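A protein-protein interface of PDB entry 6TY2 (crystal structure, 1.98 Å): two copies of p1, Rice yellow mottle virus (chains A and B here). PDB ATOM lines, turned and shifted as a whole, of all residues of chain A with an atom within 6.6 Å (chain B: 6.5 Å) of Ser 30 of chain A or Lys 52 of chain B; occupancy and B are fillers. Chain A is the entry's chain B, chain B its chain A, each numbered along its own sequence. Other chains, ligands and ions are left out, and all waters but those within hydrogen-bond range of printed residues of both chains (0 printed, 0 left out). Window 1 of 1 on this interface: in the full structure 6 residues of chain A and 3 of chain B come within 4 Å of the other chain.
Asn 19 of chain A touches Lys 52 of chain B (ND2 to NZ, 3.5 Å). Pro 28 of chain A touches Pro 42 of chain B. Pro 42 of chain B touches Ser 30 of chain A (CG to CB, 3.9 Å). Ser 30 of chain A touches Lys 52 of chain B. Leu 31 of chain A touches Tyr 53 of chain B. OH of Tyr 53 of chain B touches CG1 of Val 32 of chain A, at 3.6 Å.
The backbone carbonyl oxygen (O) of Ala 29 of chain A lies within hydrogen-bond range of the side-chain amino group (NZ) of Lys 52 of chain B (2.8 Å). The backbone carbonyl oxygen (O) of Leu 31 of chain A sits at hydrogen-bond distance from the side-chain amino group (NZ) of Lys 52 of chain B.
Of the printed residues of chain B, Asn 19 of chain A touches Lys 52. Arg 27 of chain A touches none of the printed residues of chain B. Of the printed residues of chain B, Ser 30 of chain A touches Pro 42 (3.9 Å) and Lys 52 (3.6 Å). Asp 40 of chain B touches none of the printed residues of chain A. Printed residues of chain A within 4 Å of Pro 42 of chain B: Pro 28 (3.8 Å) and Ser 30 (3.9 Å). Lys 52 of chain B touches four residues of chain A.
Of the 11 printed residues of chain A, 6 touch a printed residue of chain B. Printed residues of chain A that touch a printed residue of chain B: Asn 19, Pro 28, Ala 29, Ser 30, Leu 31 and Val 32. Hydrophobic or aromatic side chains of chain A within 4 Å of the printed part of chain B: Pro 28 and Val 32. Along chain A the printed residues that touch a printed residue of chain B span positions 19 to 32. Among the printed residues, 8 pairs touch across the chains.
Positions printed for both chains: 54 and 55. Of the 8 pairs that touch across the chains among the printed residues, none has its exchanged pair printed and touching as well.
The backbone carbonyl oxygen (O) of Leu 31 of chain A is in hydrogen-bond range of the side-chain amide nitrogen (ND2) of Asn 19 of chain A (3.1 Å). N of Val 32 of chain A sits at hydrogen-bond distance from OD1 of Asn 55 of chain A.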
ATOM      1  N   ILE A  15      14.761  19.529 -12.922  1.00  0.00           N
ATOM      2  CA  ILE A  15      16.149  19.516 -12.504  1.00  0.00           C
ATOM      3  C   ILE A  15      16.421  20.614 -11.495  1.00  0.00           C
ATOM      4  O   ILE A  15      17.116  20.393 -10.514  1.00  0.00           O
ATOM      5  CB  ILE A  15      17.101  19.702 -13.707  1.00  0.00           C
ATOM      6  CG1 ILE A  15      16.876  18.603 -14.756  1.00  0.00           C
ATOM      7  CG2 ILE A  15      18.546  19.763 -13.244  1.00  0.00           C
ATOM      8  CD1 ILE A  15      17.075  17.233 -14.248  1.00  0.00           C
ATOM      9  N   ASN A  19      17.824  19.841  -7.619  1.00  0.00           N
ATOM     10  CA  ASN A  19      19.051  20.449  -7.125  1.00  0.00           C
ATOM     11  C   ASN A  19      18.800  21.215  -5.864  1.00  0.00           C
ATOM     12  O   ASN A  19      19.548  21.085  -4.901  1.00  0.00           O
ATOM     13  CB  ASN A  19      19.671  21.387  -8.166  1.00  0.00           C
ATOM     14  CG  ASN A  19      20.506  20.646  -9.192  1.00  0.00           C
ATOM     15  OD1 ASN A  19      20.989  19.544  -8.935  1.00  0.00           O
ATOM     16  ND2 ASN A  19      20.692  21.255 -10.358  1.00  0.00           N
ATOM     17  N   ALA A  22      18.200  18.935  -3.168  1.00  0.00           N
ATOM     18  CA  ALA A  22      19.450  18.299  -2.774  1.00  0.00           C
ATOM     19  C   ALA A  22      20.242  19.231  -1.863  1.00  0.00           C
ATOM     20  O   ALA A  22      20.745  18.808  -0.825  1.00  0.00           O
ATOM     21  CB  ALA A  22      20.266  17.909  -3.997  1.00  0.00           C
ATOM     22  N   ARG A  27      23.115  17.304   0.461  1.00  0.00           N
ATOM     23  CA  ARG A  27      23.771  16.490  -0.566  1.00  0.00           C
ATOM     24  C   ARG A  27      24.300  17.395  -1.684  1.00  0.00           C
ATOM     25  O   ARG A  27      23.842  18.535  -1.833  1.00  0.00           O
ATOM     26  CB  ARG A  27      22.811  15.447  -1.145  1.00  0.00           C
ATOM     27  CG  ARG A  27      22.192  14.500  -0.126  1.00  0.00           C
ATOM     28  CD  ARG A  27      21.281  13.477  -0.809  1.00  0.00           C
ATOM     29  NE  ARG A  27      19.938  14.003  -1.067  1.00  0.00           N
ATOM     30  CZ  ARG A  27      19.475  14.339  -2.268  1.00  0.00           C
ATOM     31  NH1 ARG A  27      20.248  14.217  -3.343  1.00  0.00           N
ATOM     32  NH2 ARG A  27      18.240  14.805  -2.398  1.00  0.00           N
ATOM     33  N   PRO A  28      25.275  16.902  -2.467  1.00  0.00           N
ATOM     34  CA  PRO A  28      25.702  17.734  -3.597  1.00  0.00           C
ATOM     35  C   PRO A  28      24.590  17.867  -4.643  1.00  0.00           C
ATOM     36  O   PRO A  28      23.831  16.928  -4.905  1.00  0.00           O
ATOM     37  CB  PRO A  28      26.914  16.981  -4.164  1.00  0.00           C
ATOM     38  CG  PRO A  28      27.351  16.049  -3.065  1.00  0.00           C
ATOM     39  CD  PRO A  28      26.101  15.691  -2.323  1.00  0.00           C
ATOM     40  N   ALA A  29      24.485  19.058  -5.214  1.00  0.00           N
ATOM     41  CA  ALA A  29      23.518  19.321  -6.259  1.00  0.00           C
ATOM     42  C   ALA A  29      24.217  19.168  -7.600  1.00  0.00           C
ATOM     43  O   ALA A  29      24.756  20.134  -8.131  1.00  0.00           O
ATOM     44  CB  ALA A  29      22.929  20.714  -6.102  1.00  0.00           C
ATOM     45  N   SER A  30      24.213  17.952  -8.135  1.00  0.00           N
ATOM     46  CA  SER A  30      25.053  17.619  -9.276  1.00  0.00           C
ATOM     47  C   SER A  30      24.355  17.628 -10.636  1.00  0.00           C
ATOM     48  O   SER A  30      25.012  17.452 -11.665  1.00  0.00           O
ATOM     49  CB  SER A  30      25.684  16.242  -9.045  1.00  0.00           C
ATOM     50  OG  SER A  30      24.703  15.321  -8.587  1.00  0.00           O
ATOM     51  N   LEU A  31      23.042  17.843 -10.665  1.00  0.00           N
ATOM     52  CA  LEU A  31      22.315  17.752 -11.933  1.00  0.00           C
ATOM     53  C   LEU A  31      22.551  18.973 -12.811  1.00  0.00           C
ATOM     54  O   LEU A  31      22.727  20.081 -12.305  1.00  0.00           O
ATOM     55  CB  LEU A  31      20.816  17.567 -11.695  1.00  0.00           C
ATOM     56  CG  LEU A  31      20.291  16.201 -11.231  1.00  0.00           C
ATOM     57  CD1 LEU A  31      20.769  15.888  -9.831  1.00  0.00           C
ATOM     58  CD2 LEU A  31      18.776  16.194 -11.250  1.00  0.00           C
ATOM     59  N   VAL A  32      22.548  18.769 -14.128  1.00  0.00           N
ATOM     60  CA  VAL A  32      22.736  19.864 -15.072  1.00  0.00           C
ATOM     61  C   VAL A  32      21.552  19.970 -16.031  1.00  0.00           C
ATOM     62  O   VAL A  32      20.845  18.983 -16.280  1.00  0.00           O
ATOM     63  CB  VAL A  32      24.042  19.702 -15.872  1.00  0.00           C
ATOM     64  CG1 VAL A  32      25.226  19.656 -14.925  1.00  0.00           C
ATOM     65  CG2 VAL A  32      24.001  18.433 -16.732  1.00  0.00           C
ATOM     66  N   LEU A  54      23.658  11.141 -17.537  1.00  0.00           N
ATOM     67  CA  LEU A  54      23.995  12.544 -17.334  1.00  0.00           C
ATOM     68  C   LEU A  54      23.590  13.016 -15.931  1.00  0.00           C
ATOM     69  O   LEU A  54      24.402  13.580 -15.206  1.00  0.00           O
ATOM     70  CB  LEU A  54      23.318  13.413 -18.399  1.00  0.00           C
ATOM     71  CG  LEU A  54      23.608  14.912 -18.290  1.00  0.00           C
ATOM     72  CD1 LEU A  54      25.049  15.166 -18.649  1.00  0.00           C
ATOM     73  CD2 LEU A  54      22.647  15.750 -19.146  1.00  0.00           C
ATOM     74  N   ASN A  55      22.344  12.754 -15.544  1.00  0.00           N
ATOM     75  CA  ASN A  55      21.861  13.194 -14.249  1.00  0.00           C
ATOM     76  C   ASN A  55      21.463  12.048 -13.320  1.00  0.00           C
ATOM     77  O   ASN A  55      20.444  12.139 -12.634  1.00  0.00           O
ATOM     78  CB  ASN A  55      20.674  14.138 -14.436  1.00  0.00           C
ATOM     79  CG  ASN A  55      21.093  15.482 -14.989  1.00  0.00           C
ATOM     80  OD1 ASN A  55      22.180  15.980 -14.676  1.00  0.00           O
ATOM     81  ND2 ASN A  55      20.246  16.072 -15.836  1.00  0.00           N
ATOM     82  N   CYS B  39      37.509  21.886  -7.793  1.00  0.00           N
ATOM     83  CA  CYS B  39      37.281  20.533  -8.291  1.00  0.00           C
ATOM     84  C   CYS B  39      35.829  20.327  -8.738  1.00  0.00           C
ATOM     85  O   CYS B  39      34.912  20.820  -8.088  1.00  0.00           O
ATOM     86  CB  CYS B  39      37.661  19.551  -7.187  1.00  0.00           C
ATOM     87  SG  CYS B  39      37.188  17.875  -7.405  1.00  0.00           S
ATOM     88  N   ASP B  40      35.600  19.617  -9.836  1.00  0.00           N
ATOM     89  CA  ASP B  40      34.223  19.487 -10.311  1.00  0.00           C
ATOM     90  C   ASP B  40      33.712  18.052 -10.217  1.00  0.00           C
ATOM     91  O   ASP B  40      32.770  17.679 -10.901  1.00  0.00           O
ATOM     92  CB  ASP B  40      34.078  20.020 -11.745  1.00  0.00           C
ATOM     93  CG  ASP B  40      34.963  19.299 -12.754  1.00  0.00           C
ATOM     94  OD1 ASP B  40      35.694  18.378 -12.358  1.00  0.00           O
ATOM     95  OD2 ASP B  40      34.925  19.649 -13.961  1.00  0.00           O
ATOM     96  N   PRO B  42      31.635  15.726  -8.084  1.00  0.00           N
ATOM     97  CA  PRO B  42      30.671  15.870  -6.986  1.00  0.00           C
ATOM     98  C   PRO B  42      30.978  14.976  -5.801  1.00  0.00           C
ATOM     99  O   PRO B  42      30.782  15.389  -4.661  1.00  0.00           O
ATOM    100  CB  PRO B  42      29.342  15.471  -7.632  1.00  0.00           C
ATOM    101  CG  PRO B  42      29.544  15.754  -9.081  1.00  0.00           C
ATOM    102  CD  PRO B  42      30.974  15.391  -9.352  1.00  0.00           C
ATOM    103  N   ARG B  49      37.001  21.635  -2.873  1.00  0.00           N
ATOM    104  CA  ARG B  49      36.093  22.746  -3.128  1.00  0.00           C
ATOM    105  C   ARG B  49      35.330  22.458  -4.399  1.00  0.00           C
ATOM    106  O   ARG B  49      35.909  22.433  -5.478  1.00  0.00           O
ATOM    107  CB  ARG B  49      36.839  24.062  -3.260  1.00  0.00           C
ATOM    108  CG  ARG B  49      35.916  25.260  -3.392  1.00  0.00           C
ATOM    109  CD  ARG B  49      36.701  26.549  -3.321  1.00  0.00           C
ATOM    110  NE  ARG B  49      35.827  27.712  -3.361  1.00  0.00           N
ATOM    111  CZ  ARG B  49      36.244  28.962  -3.188  1.00  0.00           C
ATOM    112  NH1 ARG B  49      37.528  29.209  -2.958  1.00  0.00           N
ATOM    113  NH2 ARG B  49      35.375  29.960  -3.243  1.00  0.00           N
ATOM    114  N   PHE B  50      34.031  22.243  -4.276  1.00  0.00           N
ATOM    115  CA  PHE B  50      33.237  21.830  -5.417  1.00  0.00           C
ATOM    116  C   PHE B  50      32.851  23.042  -6.245  1.00  0.00           C
ATOM    117  O   PHE B  50      32.141  23.940  -5.792  1.00  0.00           O
ATOM    118  CB  PHE B  50      32.005  21.053  -4.958  1.00  0.00           C
ATOM    119  CG  PHE B  50      31.176  20.495  -6.077  1.00  0.00           C
ATOM    120  CD1 PHE B  50      31.763  19.800  -7.113  1.00  0.00           C
ATOM    121  CD2 PHE B  50      29.803  20.649  -6.073  1.00  0.00           C
ATOM    122  CE1 PHE B  50      31.002  19.283  -8.139  1.00  0.00           C
ATOM    123  CE2 PHE B  50      29.030  20.134  -7.090  1.00  0.00           C
ATOM    124  CZ  PHE B  50      29.629  19.450  -8.126  1.00  0.00           C
ATOM    125  N   VAL B  51      33.354  23.050  -7.469  1.00  0.00           N
ATOM    126  CA  VAL B  51      33.128  24.104  -8.430  1.00  0.00           C
ATOM    127  C   VAL B  51      32.479  23.431  -9.616  1.00  0.00           C
ATOM    128  O   VAL B  51      33.166  22.923 -10.504  1.00  0.00           O
ATOM    129  CB  VAL B  51      34.439  24.792  -8.819  1.00  0.00           C
ATOM    130  CG1 VAL B  51      34.196  25.870  -9.878  1.00  0.00           C
ATOM    131  CG2 VAL B  51      35.082  25.370  -7.568  1.00  0.00           C
ATOM    132  N   LYS B  52      31.148  23.410  -9.597  1.00  0.00           N
ATOM    133  CA  LYS B  52      30.370  22.462 -10.380  1.00  0.00           C
ATOM    134  C   LYS B  52      30.578  22.589 -11.888  1.00  0.00           C
ATOM    135  O   LYS B  52      30.569  21.590 -12.615  1.00  0.00           O
ATOM    136  CB  LYS B  52      28.893  22.632 -10.056  1.00  0.00           C
ATOM    137  CG  LYS B  52      27.986  21.643 -10.749  1.00  0.00           C
ATOM    138  CD  LYS B  52      26.537  21.969 -10.414  1.00  0.00           C
ATOM    139  CE  LYS B  52      25.572  21.001 -11.038  1.00  0.00           C
ATOM    140  NZ  LYS B  52      24.186  21.354 -10.579  1.00  0.00           N
ATOM    141  N   TYR B  53      30.758  23.821 -12.344  1.00  0.00           N
ATOM    142  CA  TYR B  53      30.846  24.100 -13.766  1.00  0.00           C
ATOM    143  C   TYR B  53      32.236  24.598 -14.144  1.00  0.00           C
ATOM    144  O   TYR B  53      32.410  25.410 -15.053  1.00  0.00           O
ATOM    145  CB  TYR B  53      29.780  25.105 -14.152  1.00  0.00           C
ATOM    146  CG  TYR B  53      28.376  24.554 -14.040  1.00  0.00           C
ATOM    147  CD1 TYR B  53      27.861  23.755 -15.036  1.00  0.00           C
ATOM    148  CD2 TYR B  53      27.578  24.834 -12.938  1.00  0.00           C
ATOM    149  CE1 TYR B  53      26.591  23.255 -14.965  1.00  0.00           C
ATOM    150  CE2 TYR B  53      26.282  24.334 -12.845  1.00  0.00           C
ATOM    151  CZ  TYR B  53      25.800  23.542 -13.872  1.00  0.00           C
ATOM    152  OH  TYR B  53      24.533  23.026 -13.837  1.00  0.00           O
ATOM    153  N   LEU B  54      33.221  24.065 -13.437  1.00  0.00           N
ATOM    154  CA  LEU B  54      34.624  24.368 -13.680  1.00  0.00           C
ATOM    155  C   LEU B  54      34.954  24.188 -15.153  1.00  0.00           C
ATOM    156  O   LEU B  54      35.692  24.972 -15.727  1.00  0.00           O
ATOM    157  CB  LEU B  54      35.504  23.464 -12.811  1.00  0.00           C
ATOM    158  CG  LEU B  54      37.020  23.613 -12.773  1.00  0.00           C
ATOM    159  CD1 LEU B  54      37.431  24.935 -12.146  1.00  0.00           C
ATOM    160  CD2 LEU B  54      37.626  22.450 -12.011  1.00  0.00           C
ATOM    161  N   ASN B  55      34.364  23.168 -15.764  1.00  0.00           N
ATOM    162  CA  ASN B  55      34.616  22.875 -17.162  1.00  0.00           C
ATOM    163  C   ASN B  55      33.375  22.874 -18.068  1.00  0.00           C
ATOM    164  O   ASN B  55      32.515  21.993 -17.965  1.00  0.00           O
ATOM    165  CB  ASN B  55      35.345  21.531 -17.245  1.00  0.00           C
ATOM    166  CG  ASN B  55      36.809  21.656 -16.859  1.00  0.00           C
ATOM    167  OD1 ASN B  55      37.494  22.548 -17.336  1.00  0.00           O
ATOM    168  ND2 ASN B  55      37.276  20.798 -15.972  1.00  0.00           N
